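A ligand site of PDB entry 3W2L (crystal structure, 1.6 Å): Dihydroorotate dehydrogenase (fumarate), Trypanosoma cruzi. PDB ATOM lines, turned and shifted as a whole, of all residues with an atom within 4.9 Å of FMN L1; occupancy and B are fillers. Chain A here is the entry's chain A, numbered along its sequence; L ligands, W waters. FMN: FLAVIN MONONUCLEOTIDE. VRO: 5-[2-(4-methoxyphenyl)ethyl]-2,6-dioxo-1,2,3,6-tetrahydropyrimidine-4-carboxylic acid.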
ATOM      1  N   ALA A  19      19.772  20.729 -32.187  1.00  0.00           N
ATOM      2  CA  ALA A  19      21.045  20.186 -31.803  1.00  0.00           C
ATOM      3  C   ALA A  19      20.925  19.023 -30.819  1.00  0.00           C
ATOM      4  O   ALA A  19      20.008  19.021 -30.033  1.00  0.00           O
ATOM      5  CB  ALA A  19      21.888  21.286 -31.186  1.00  0.00           C
ATOM      6  N   ALA A  20      21.719  17.966 -30.987  1.00  0.00           N
ATOM      7  CA  ALA A  20      21.570  16.830 -30.129  1.00  0.00           C
ATOM      8  C   ALA A  20      21.668  17.295 -28.694  1.00  0.00           C
ATOM      9  O   ALA A  20      22.434  18.165 -28.360  1.00  0.00           O
ATOM     10  CB  ALA A  20      22.571  15.725 -30.483  1.00  0.00           C
ATOM     11  N   GLY A  21      20.809  16.714 -27.858  1.00  0.00           N
ATOM     12  CA  GLY A  21      20.797  16.991 -26.460  1.00  0.00           C
ATOM     13  C   GLY A  21      19.648  17.925 -26.128  1.00  0.00           C
ATOM     14  O   GLY A  21      19.206  17.971 -24.943  1.00  0.00           O
ATOM     15  N   VAL A  22      19.175  18.716 -27.080  1.00  0.00           N
ATOM     16  CA  VAL A  22      18.095  19.665 -26.788  1.00  0.00           C
ATOM     17  C   VAL A  22      16.744  19.196 -27.336  1.00  0.00           C
ATOM     18  O   VAL A  22      16.635  18.871 -28.435  1.00  0.00           O
ATOM     19  CB  VAL A  22      18.446  21.054 -27.350  1.00  0.00           C
ATOM     20  CG1 VAL A  22      17.346  22.075 -27.135  1.00  0.00           C
ATOM     21  CG2 VAL A  22      19.744  21.482 -26.772  1.00  0.00           C
ATOM     22  N   LYS A  44      18.711  12.532 -28.526  1.00  0.00           N
ATOM     23  CA  LYS A  44      19.725  12.654 -27.496  1.00  0.00           C
ATOM     24  C   LYS A  44      20.819  11.582 -27.667  1.00  0.00           C
ATOM     25  O   LYS A  44      20.531  10.447 -27.815  1.00  0.00           O
ATOM     26  CB  LYS A  44      19.104  12.520 -26.100  1.00  0.00           C
ATOM     27  CG  LYS A  44      20.060  12.491 -24.953  1.00  0.00           C
ATOM     28  CD  LYS A  44      20.901  13.739 -24.739  1.00  0.00           C
ATOM     29  CE  LYS A  44      22.096  13.525 -23.765  1.00  0.00           C
ATOM     30  NZ  LYS A  44      22.951  14.825 -23.510  1.00  0.00           N
ATOM     31  N   SER A  45      22.058  12.030 -27.621  1.00  0.00           N
ATOM     32  CA  SER A  45      23.223  11.109 -27.631  1.00  0.00           C
ATOM     33  C   SER A  45      22.990  10.055 -26.580  1.00  0.00           C
ATOM     34  O   SER A  45      22.675  10.357 -25.471  1.00  0.00           O
ATOM     35  CB  SER A  45      24.548  11.749 -27.391  1.00  0.00           C
ATOM     36  OG  SER A  45      24.927  12.610 -28.447  1.00  0.00           O
ATOM     37  N   TYR A  59      22.589  22.665 -16.214  1.00  0.00           N
ATOM     38  CA  TYR A  59      22.416  23.566 -17.326  1.00  0.00           C
ATOM     39  C   TYR A  59      21.950  24.913 -16.820  1.00  0.00           C
ATOM     40  O   TYR A  59      21.032  24.970 -15.934  1.00  0.00           O
ATOM     41  CB  TYR A  59      21.399  23.027 -18.274  1.00  0.00           C
ATOM     42  CG  TYR A  59      20.969  24.002 -19.404  1.00  0.00           C
ATOM     43  CD1 TYR A  59      21.672  24.128 -20.600  1.00  0.00           C
ATOM     44  CD2 TYR A  59      19.882  24.871 -19.220  1.00  0.00           C
ATOM     45  CE1 TYR A  59      21.305  25.038 -21.579  1.00  0.00           C
ATOM     46  CE2 TYR A  59      19.566  25.810 -20.131  1.00  0.00           C
ATOM     47  CZ  TYR A  59      20.203  25.873 -21.343  1.00  0.00           C
ATOM     48  OH  TYR A  59      19.877  26.755 -22.346  1.00  0.00           O
ATOM     49  N   SER A  66      24.810  29.634 -22.937  1.00  0.00           N
ATOM     50  CA  SER A  66      24.522  28.645 -21.951  1.00  0.00           C
ATOM     51  C   SER A  66      25.804  27.899 -21.569  1.00  0.00           C
ATOM     52  O   SER A  66      26.822  27.909 -22.281  1.00  0.00           O
ATOM     53  CB  SER A  66      23.506  27.618 -22.456  1.00  0.00           C
ATOM     54  OG  SER A  66      24.085  26.837 -23.494  1.00  0.00           O
ATOM     55  N   ASN A  68      26.730  23.913 -19.751  1.00  0.00           N
ATOM     56  CA  ASN A  68      26.172  22.616 -19.339  1.00  0.00           C
ATOM     57  C   ASN A  68      27.191  21.580 -19.037  1.00  0.00           C
ATOM     58  O   ASN A  68      28.222  21.484 -19.676  1.00  0.00           O
ATOM     59  CB  ASN A  68      25.160  22.060 -20.346  1.00  0.00           C
ATOM     60  CG  ASN A  68      25.797  21.172 -21.416  1.00  0.00           C
ATOM     61  OD1 ASN A  68      26.082  19.961 -21.227  1.00  0.00           O
ATOM     62  ND2 ASN A  68      26.064  21.766 -22.582  1.00  0.00           N
ATOM     63  N   MET A  70      25.789  18.173 -18.494  1.00  0.00           N
ATOM     64  CA  MET A  70      24.679  17.238 -18.272  1.00  0.00           C
ATOM     65  C   MET A  70      25.127  15.853 -17.808  1.00  0.00           C
ATOM     66  O   MET A  70      24.434  15.187 -17.021  1.00  0.00           O
ATOM     67  CB  MET A  70      23.879  17.123 -19.546  1.00  0.00           C
ATOM     68  CG  MET A  70      23.304  18.407 -20.110  1.00  0.00           C
ATOM     69  SD  MET A  70      22.284  19.355 -19.034  1.00  0.00           S
ATOM     70  CE  MET A  70      20.833  18.376 -19.051  1.00  0.00           C
ATOM     71  N   LEU A  72      25.539  13.199 -20.006  1.00  0.00           N
ATOM     72  CA  LEU A  72      24.857  12.248 -20.845  1.00  0.00           C
ATOM     73  C   LEU A  72      23.657  11.538 -20.230  1.00  0.00           C
ATOM     74  O   LEU A  72      23.493  10.311 -20.343  1.00  0.00           O
ATOM     75  CB  LEU A  72      25.877  11.248 -21.373  1.00  0.00           C
ATOM     76  CG  LEU A  72      25.810  10.639 -22.738  1.00  0.00           C
ATOM     77  CD1 LEU A  72      25.491  11.516 -23.912  1.00  0.00           C
ATOM     78  CD2 LEU A  72      27.240  10.006 -22.903  1.00  0.00           C
ATOM     79  N   SER A  98      21.727  10.070 -32.553  1.00  0.00           N
ATOM     80  CA  SER A  98      23.086  10.332 -32.120  1.00  0.00           C
ATOM     81  C   SER A  98      23.503   9.271 -31.093  1.00  0.00           C
ATOM     82  O   SER A  98      22.750   8.923 -30.292  1.00  0.00           O
ATOM     83  CB  SER A  98      23.144  11.698 -31.452  1.00  0.00           C
ATOM     84  OG  SER A  98      24.407  11.943 -30.924  1.00  0.00           O
ATOM     85  N   GLU A 126      24.440   9.865 -36.338  1.00  0.00           N
ATOM     86  CA  GLU A 126      25.399  10.944 -35.928  1.00  0.00           C
ATOM     87  C   GLU A 126      26.221  10.379 -34.787  1.00  0.00           C
ATOM     88  O   GLU A 126      25.746  10.161 -33.675  1.00  0.00           O
ATOM     89  CB  GLU A 126      24.700  12.285 -35.555  1.00  0.00           C
ATOM     90  CG  GLU A 126      25.711  13.443 -35.299  1.00  0.00           C
ATOM     91  CD  GLU A 126      25.016  14.833 -35.098  1.00  0.00           C
ATOM     92  OE1 GLU A 126      24.624  15.098 -33.945  1.00  0.00           O
ATOM     93  OE2 GLU A 126      24.821  15.685 -36.052  1.00  0.00           O
ATOM     94  N   ASN A 128      28.848  10.917 -32.007  1.00  0.00           N
ATOM     95  CA  ASN A 128      29.404  11.992 -31.270  1.00  0.00           C
ATOM     96  C   ASN A 128      30.819  11.692 -30.821  1.00  0.00           C
ATOM     97  O   ASN A 128      31.036  10.887 -29.996  1.00  0.00           O
ATOM     98  CB  ASN A 128      28.544  12.199 -30.032  1.00  0.00           C
ATOM     99  CG  ASN A 128      28.961  13.393 -29.178  1.00  0.00           C
ATOM    100  OD1 ASN A 128      29.803  14.103 -29.473  1.00  0.00           O
ATOM    101  ND2 ASN A 128      28.289  13.547 -28.099  1.00  0.00           N
ATOM    102  N   LYS A 165      29.729  14.225 -35.133  1.00  0.00           N
ATOM    103  CA  LYS A 165      29.590  15.494 -34.430  1.00  0.00           C
ATOM    104  C   LYS A 165      30.990  15.820 -33.797  1.00  0.00           C
ATOM    105  O   LYS A 165      31.588  15.014 -33.022  1.00  0.00           O
ATOM    106  CB  LYS A 165      28.600  15.345 -33.285  1.00  0.00           C
ATOM    107  CG  LYS A 165      28.419  16.587 -32.437  1.00  0.00           C
ATOM    108  CD  LYS A 165      27.644  17.685 -33.097  1.00  0.00           C
ATOM    109  CE  LYS A 165      27.188  18.747 -32.146  1.00  0.00           C
ATOM    110  NZ  LYS A 165      26.059  18.365 -31.307  1.00  0.00           N
ATOM    111  N   VAL A 194      29.572  22.803 -34.618  1.00  0.00           N
ATOM    112  CA  VAL A 194      30.393  22.206 -33.602  1.00  0.00           C
ATOM    113  C   VAL A 194      29.578  21.814 -32.373  1.00  0.00           C
ATOM    114  O   VAL A 194      28.531  22.298 -32.154  1.00  0.00           O
ATOM    115  CB  VAL A 194      31.481  23.177 -33.087  1.00  0.00           C
ATOM    116  CG1 VAL A 194      32.441  23.502 -34.177  1.00  0.00           C
ATOM    117  CG2 VAL A 194      30.839  24.467 -32.619  1.00  0.00           C
ATOM    118  N   ASN A 195      30.153  20.928 -31.580  1.00  0.00           N
ATOM    119  CA  ASN A 195      29.672  20.723 -30.210  1.00  0.00           C
ATOM    120  C   ASN A 195      30.072  21.939 -29.318  1.00  0.00           C
ATOM    121  O   ASN A 195      30.640  22.845 -29.788  1.00  0.00           O
ATOM    122  CB  ASN A 195      30.297  19.422 -29.697  1.00  0.00           C
ATOM    123  CG  ASN A 195      29.437  18.698 -28.692  1.00  0.00           C
ATOM    124  OD1 ASN A 195      28.943  19.272 -27.847  1.00  0.00           O
ATOM    125  ND2 ASN A 195      29.327  17.430 -28.844  1.00  0.00           N
ATOM    126  N   SER A 196      29.741  21.888 -28.035  1.00  0.00           N
ATOM    127  CA  SER A 196      29.973  23.030 -27.204  1.00  0.00           C
ATOM    128  C   SER A 196      31.453  23.370 -27.073  1.00  0.00           C
ATOM    129  O   SER A 196      32.268  22.530 -27.266  1.00  0.00           O
ATOM    130  CB  SER A 196      29.361  22.764 -25.808  1.00  0.00           C
ATOM    131  OG  SER A 196      29.713  21.579 -25.337  1.00  0.00           O
ATOM    132  N   GLY A 222      27.581  27.175 -25.075  1.00  0.00           N
ATOM    133  CA  GLY A 222      26.797  27.306 -26.257  1.00  0.00           C
ATOM    134  C   GLY A 222      26.288  28.712 -26.393  1.00  0.00           C
ATOM    135  O   GLY A 222      26.339  29.487 -25.458  1.00  0.00           O
ATOM    136  N   GLY A 223      25.681  29.010 -27.517  1.00  0.00           N
ATOM    137  CA  GLY A 223      24.948  30.221 -27.743  1.00  0.00           C
ATOM    138  C   GLY A 223      25.794  31.347 -28.419  1.00  0.00           C
ATOM    139  O   GLY A 223      26.708  31.093 -29.184  1.00  0.00           O
ATOM    140  N   ILE A 226      29.648  31.550 -29.012  1.00  0.00           N
ATOM    141  CA  ILE A 226      30.393  30.547 -29.829  1.00  0.00           C
ATOM    142  C   ILE A 226      30.150  30.663 -31.351  1.00  0.00           C
ATOM    143  O   ILE A 226      30.709  29.907 -32.101  1.00  0.00           O
ATOM    144  CB  ILE A 226      30.164  29.079 -29.394  1.00  0.00           C
ATOM    145  CG1 ILE A 226      28.816  28.496 -29.884  1.00  0.00           C
ATOM    146  CG2 ILE A 226      30.308  28.923 -27.879  1.00  0.00           C
ATOM    147  CD1 ILE A 226      28.763  26.972 -29.858  1.00  0.00           C
ATOM    148  N   CYS A 249      26.370  23.994 -36.438  1.00  0.00           N
ATOM    149  CA  CYS A 249      25.734  24.088 -35.102  1.00  0.00           C
ATOM    150  C   CYS A 249      26.558  25.068 -34.278  1.00  0.00           C
ATOM    151  O   CYS A 249      27.786  24.992 -34.285  1.00  0.00           O
ATOM    152  CB  CYS A 249      25.747  22.713 -34.481  1.00  0.00           C
ATOM    153  SG  CYS A 249      24.842  22.636 -32.920  1.00  0.00           S
ATOM    154  N   GLY A 250      25.919  26.036 -33.641  1.00  0.00           N
ATOM    155  CA  GLY A 250      26.522  26.943 -32.701  1.00  0.00           C
ATOM    156  C   GLY A 250      26.075  28.348 -32.929  1.00  0.00           C
ATOM    157  O   GLY A 250      26.320  28.936 -33.961  1.00  0.00           O
ATOM    158  N   GLY A 251      25.490  28.897 -31.882  1.00  0.00           N
ATOM    159  CA  GLY A 251      25.118  30.304 -31.937  1.00  0.00           C
ATOM    160  C   GLY A 251      24.033  30.725 -32.793  1.00  0.00           C
ATOM    161  O   GLY A 251      23.954  31.946 -33.041  1.00  0.00           O
ATOM    162  N   VAL A 252      23.185  29.817 -33.275  1.00  0.00           N
ATOM    163  CA  VAL A 252      22.072  30.225 -34.118  1.00  0.00           C
ATOM    164  C   VAL A 252      20.915  30.694 -33.234  1.00  0.00           C
ATOM    165  O   VAL A 252      20.317  29.932 -32.534  1.00  0.00           O
ATOM    166  CB  VAL A 252      21.629  29.114 -35.092  1.00  0.00           C
ATOM    167  CG1 VAL A 252      20.401  29.506 -35.918  1.00  0.00           C
ATOM    168  CG2 VAL A 252      22.804  28.720 -35.989  1.00  0.00           C
ATOM    169  N   GLN A 270      21.730  23.400 -37.164  1.00  0.00           N
ATOM    170  CA  GLN A 270      21.207  22.927 -35.911  1.00  0.00           C
ATOM    171  C   GLN A 270      21.152  24.060 -34.838  1.00  0.00           C
ATOM    172  O   GLN A 270      21.875  24.951 -34.866  1.00  0.00           O
ATOM    173  CB  GLN A 270      22.102  21.778 -35.404  1.00  0.00           C
ATOM    174  CG  GLN A 270      22.421  20.699 -36.402  1.00  0.00           C
ATOM    175  CD  GLN A 270      23.088  19.509 -35.740  1.00  0.00           C
ATOM    176  OE1 GLN A 270      23.688  19.618 -34.699  1.00  0.00           O
ATOM    177  NE2 GLN A 270      22.995  18.399 -36.365  1.00  0.00           N
ATOM    178  N   VAL A 271      20.155  23.945 -33.966  1.00  0.00           N
ATOM    179  CA  VAL A 271      19.809  24.945 -33.013  1.00  0.00           C
ATOM    180  C   VAL A 271      19.758  24.304 -31.635  1.00  0.00           C
ATOM    181  O   VAL A 271      18.870  23.442 -31.386  1.00  0.00           O
ATOM    182  CB  VAL A 271      18.473  25.623 -33.376  1.00  0.00           C
ATOM    183  CG1 VAL A 271      18.286  26.764 -32.418  1.00  0.00           C
ATOM    184  CG2 VAL A 271      18.452  26.077 -34.855  1.00  0.00           C
ATOM    185  N   GLY A 272      20.632  24.707 -30.718  1.00  0.00           N
ATOM    186  CA  GLY A 272      20.752  24.136 -29.357  1.00  0.00           C
ATOM    187  C   GLY A 272      20.187  25.146 -28.386  1.00  0.00           C
ATOM    188  O   GLY A 272      18.975  25.169 -28.100  1.00  0.00           O
ATOM    189  N   THR A 273      21.062  25.977 -27.841  1.00  0.00           N
ATOM    190  CA  THR A 273      20.727  26.905 -26.739  1.00  0.00           C
ATOM    191  C   THR A 273      19.470  27.714 -27.092  1.00  0.00           C
ATOM    192  O   THR A 273      18.593  27.831 -26.278  1.00  0.00           O
ATOM    193  CB  THR A 273      21.902  27.872 -26.473  1.00  0.00           C
ATOM    194  OG1 THR A 273      23.067  27.146 -26.027  1.00  0.00           O
ATOM    195  CG2 THR A 273      21.637  28.931 -25.447  1.00  0.00           C
ATOM    196  N   ALA A 274      19.402  28.289 -28.267  1.00  0.00           N
ATOM    197  CA  ALA A 274      18.256  29.162 -28.583  1.00  0.00           C
ATOM    198  C   ALA A 274      16.958  28.397 -28.552  1.00  0.00           C
ATOM    199  O   ALA A 274      15.939  28.937 -28.197  1.00  0.00           O
ATOM    200  CB  ALA A 274      18.449  29.825 -29.920  1.00  0.00           C
HETATM  201  N1  FMN L   1      25.767  17.531 -28.289  1.00  0.00           N
HETATM  202  C2  FMN L   1      25.774  16.222 -28.586  1.00  0.00           C
HETATM  203  O2  FMN L   1      26.306  15.920 -29.692  1.00  0.00           O
HETATM  204  N3  FMN L   1      25.135  15.307 -27.869  1.00  0.00           N
HETATM  205  C4  FMN L   1      24.419  15.623 -26.744  1.00  0.00           C
HETATM  206  O4  FMN L   1      23.801  14.731 -26.052  1.00  0.00           O
HETATM  207  C4A FMN L   1      24.406  16.986 -26.341  1.00  0.00           C
HETATM  208  N5  FMN L   1      23.747  17.317 -25.221  1.00  0.00           N
HETATM  209  C5A FMN L   1      23.614  18.687 -24.941  1.00  0.00           C
HETATM  210  C6  FMN L   1      22.716  19.073 -23.918  1.00  0.00           C
HETATM  211  C7  FMN L   1      22.555  20.428 -23.612  1.00  0.00           C
HETATM  212  C7M FMN L   1      21.701  20.843 -22.450  1.00  0.00           C
HETATM  213  C8  FMN L   1      23.198  21.428 -24.455  1.00  0.00           C
HETATM  214  C8M FMN L   1      23.031  22.904 -24.171  1.00  0.00           C
HETATM  215  C9  FMN L   1      24.021  21.041 -25.507  1.00  0.00           C
HETATM  216  C9A FMN L   1      24.223  19.683 -25.799  1.00  0.00           C
HETATM  217  N10 FMN L   1      25.077  19.241 -26.829  1.00  0.00           N
HETATM  218  C10 FMN L   1      25.116  17.928 -27.197  1.00  0.00           C
HETATM  219  C1' FMN L   1      25.711  20.196 -27.734  1.00  0.00           C
HETATM  220  C2' FMN L   1      24.780  20.823 -28.720  1.00  0.00           C
HETATM  221  O2' FMN L   1      24.327  19.789 -29.571  1.00  0.00           O
HETATM  222  C3' FMN L   1      25.434  21.926 -29.494  1.00  0.00           C
HETATM  223  O3' FMN L   1      26.534  21.329 -30.209  1.00  0.00           O
HETATM  224  C4' FMN L   1      25.967  23.077 -28.614  1.00  0.00           C
HETATM  225  O4' FMN L   1      24.971  23.425 -27.612  1.00  0.00           O
HETATM  226  C5' FMN L   1      26.168  24.336 -29.493  1.00  0.00           C
HETATM  227  O5' FMN L   1      25.078  24.822 -30.185  1.00  0.00           O
HETATM  228  P   FMN L   1      24.270  26.113 -29.664  1.00  0.00           P
HETATM  229  O1P FMN L   1      23.066  26.254 -30.554  1.00  0.00           O
HETATM  230  O2P FMN L   1      25.231  27.273 -29.650  1.00  0.00           O
HETATM  231  O3P FMN L   1      23.860  25.772 -28.202  1.00  0.00           O
HETATM  232  OAB VRO L   2      25.514  15.234 -21.962  1.00  0.00           O
HETATM  233  CAO VRO L   2      26.344  16.164 -22.041  1.00  0.00           C
HETATM  234  OAE VRO L   2      26.887  16.654 -21.036  1.00  0.00           O
HETATM  235  CAR VRO L   2      26.826  16.729 -23.356  1.00  0.00           C
HETATM  236  NAL VRO L   2      26.843  18.148 -23.381  1.00  0.00           N
HETATM  237  CAT VRO L   2      27.359  18.851 -24.466  1.00  0.00           C
HETATM  238  OAC VRO L   2      27.426  20.095 -24.495  1.00  0.00           O
HETATM  239  NAM VRO L   2      27.784  18.047 -25.509  1.00  0.00           N
HETATM  240  CAU VRO L   2      27.831  16.638 -25.517  1.00  0.00           C
HETATM  241  OAD VRO L   2      28.262  16.045 -26.508  1.00  0.00           O
HETATM  242  CAS VRO L   2      27.381  15.978 -24.355  1.00  0.00           C
HETATM  243  CAK VRO L   2      27.398  14.563 -24.315  1.00  0.00           C
HETATM  244  CAJ VRO L   2      28.863  13.956 -24.255  1.00  0.00           C
HETATM  245  CAP VRO L   2      29.391  14.256 -23.008  1.00  0.00           C
HETATM  246  CAF VRO L   2      29.264  13.392 -21.984  1.00  0.00           C
HETATM  247  CAH VRO L   2      29.754  13.621 -20.674  1.00  0.00           C
HETATM  248  CAQ VRO L   2      30.357  14.841 -20.397  1.00  0.00           C
HETATM  249  OAN VRO L   2      30.840  15.080 -19.115  1.00  0.00           O
HETATM  250  CAA VRO L   2      31.879  16.120 -18.957  1.00  0.00           C
HETATM  251  CAI VRO L   2      30.495  15.789 -21.448  1.00  0.00           C
HETATM  252  CAG VRO L   2      30.010  15.493 -22.750  1.00  0.00           C
HETATM  253  O   HOH W   1      25.748  14.026 -31.724  1.00  0.00           O
HETATM  254  O   HOH W   2      23.180  26.754 -33.214  1.00  0.00           O
HETATM  255  O   HOH W   3      21.475  28.399 -30.272  1.00  0.00           O
HETATM  256  O   HOH W   4      20.610  16.667 -22.557  1.00  0.00           O
HETATM  257  O   HOH W   5      26.439  23.751 -25.668  1.00  0.00           O
HETATM  258  O   HOH W   6      25.775  24.680 -22.921  1.00  0.00           O
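The side-chain hydroxyl (OG) of Ser 66 lies within hydrogen-bond range of the side-chain hydroxyl (OG1) of Thr 273 (2.7 Å). OG of Ser 98 is in hydrogen-bond range of OG of Ser 45 (2.6 Å). The backbone NH (N) of Val 194 is in hydrogen-bond range of the backbone carbonyl oxygen (O) of Cys 249. The side-chain amide nitrogen (ND2) of Asn 195 lies within hydrogen-bond range of the side-chain amide oxygen (OD1) of Asn 128, 3.4 Å away. OD1 of Asn 195 sits at hydrogen-bond distance from OG of Ser 196, 3.5 Å away. The backbone NH (N) of Ala 19 is in hydrogen-bond range of the backbone carbonyl oxygen (O) of Val 271, at 3.0 Å. The side-chain sulfur of Cys 249 is in hydrogen-bond range of the side-chain amide oxygen of Gln 270. O of Gly 222 is in hydrogen-bond range of N of Ser 66, 3.0 Å away.
NZ of Lys 44 lies within hydrogen-bond range of O4 of FMN L1. An oxygen (O3P) of FMN L1 lies within hydrogen-bond range of the backbone NH of Thr 273 (2.8 Å). OG1 of Thr 273 lies within hydrogen-bond range of O3P of FMN L1, 2.7 Å away. N3 of FMN L1 lies within hydrogen-bond range of OG of Ser 45, 2.8 Å away. The backbone NH (N) of Gly 251 is in hydrogen-bond range of an oxygen (O2P) of FMN L1 (2.8 Å). N of Ala 20 lies within hydrogen-bond range of O2' of FMN L1 (3.5 Å). An oxygen (O2') of FMN L1 sits at hydrogen-bond distance from the backbone carbonyl oxygen (O) of Ala 20 (2.8 Å). An oxygen (O2P) of FMN L1 lies within hydrogen-bond range of the backbone NH of Gly 223, 2.8 Å away. An oxygen (O2') of FMN L1 lies within hydrogen-bond range of the side-chain amino group of Lys 165. N of Gly 272 is in hydrogen-bond range of O1P of FMN L1 (2.9 Å). The backbone carbonyl oxygen (O) of Val 194 is in hydrogen-bond range of an oxygen (O3') of FMN L1, 3.0 Å away. The side-chain amide nitrogen (ND2) of Asn 195 sits at hydrogen-bond distance from an oxygen (O2) of FMN L1 (3.5 Å). The side-chain sulfur (SG) of Cys 249 is in hydrogen-bond range of an oxygen (O3') of FMN L1. An oxygen (O2) of FMN L1 is in hydrogen-bond range of the side-chain amide nitrogen (ND2) of Asn 128, 3.5 Å away. The side-chain amino group of Lys 44 is in salt-bridge range of an oxygen (OAB) of VRO L2 (3.0 Å). A nitrogen (NAM) of VRO L2 lies within hydrogen-bond range of the side-chain amide oxygen of Asn 195, 2.9 Å away. An oxygen (OAC) of VRO L2 is in hydrogen-bond range of the side-chain amide nitrogen of Asn 68 (2.9 Å). OAD of VRO L2 is in hydrogen-bond range of ND2 of Asn 128 (3.0 Å). An oxygen (OAE) of VRO L2 lies within hydrogen-bond range of the backbone NH (N) of Met 70 (3.2 Å). An oxygen (OAC) of VRO L2 lies within hydrogen-bond range of the side-chain hydroxyl (OG) of Ser 196, 2.9 Å away. N of Leu 72 is in hydrogen-bond range of OAB of VRO L2, at 2.8 Å.
Merely in contact with FMN L1: Ala 19 (3.3 Å), Gly 21 (3.2 Å), Tyr 59 (3.8 Å), Asn 68 (3.4 Å), Met 70 (3.7 Å), Ser 196 (3.9 Å), Gly 222 (3.7 Å), Ile 226 (3.6 Å), Gly 250 (3.3 Å) and Val 271 (3.99 Å). Hydrophobic or aromatic side chains that line FMN L1: Ala 19, Ala 20, Tyr 59, Met 70 and Ile 226. Within 4 Å of FMN L1: Ala 19, Ala 20, Gly 21, Lys 44, Ser 45, Tyr 59, Asn 68, Met 70, Asn 128, Lys 165, Val 194, Asn 195, Ser 196, Gly 222, Gly 223, Ile 226, Cys 249, Gly 250, Gly 251, Val 271, Gly 272 and Thr 273.
Water W3 lies within hydrogen-bond range of an oxygen (O1P) of FMN L1 (2.7 Å), the backbone NH of Ala 274 (2.9 Å), the backbone carbonyl oxygen of Val 252 (3.0 Å) and the backbone NH of Thr 273 (3.5 Å). Water W1 lies within hydrogen-bond range of OG of Ser 98 (2.6 Å), OE1 of Glu 126 (2.7 Å) and O2 of FMN L1 (2.8 Å). Water W4 lies within hydrogen-bond range of O of Gly 21 (3.1 Å) and NZ of Lys 44 (3.1 Å). Water W6 bridges OG of Ser 66 (2.8 Å) and ND2 of Asn 68 (2.9 Å).
A nitrogen (N1) of FMN L1 sits close to a nitrogen (NAM) of VRO L2, 3.5 Å away.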
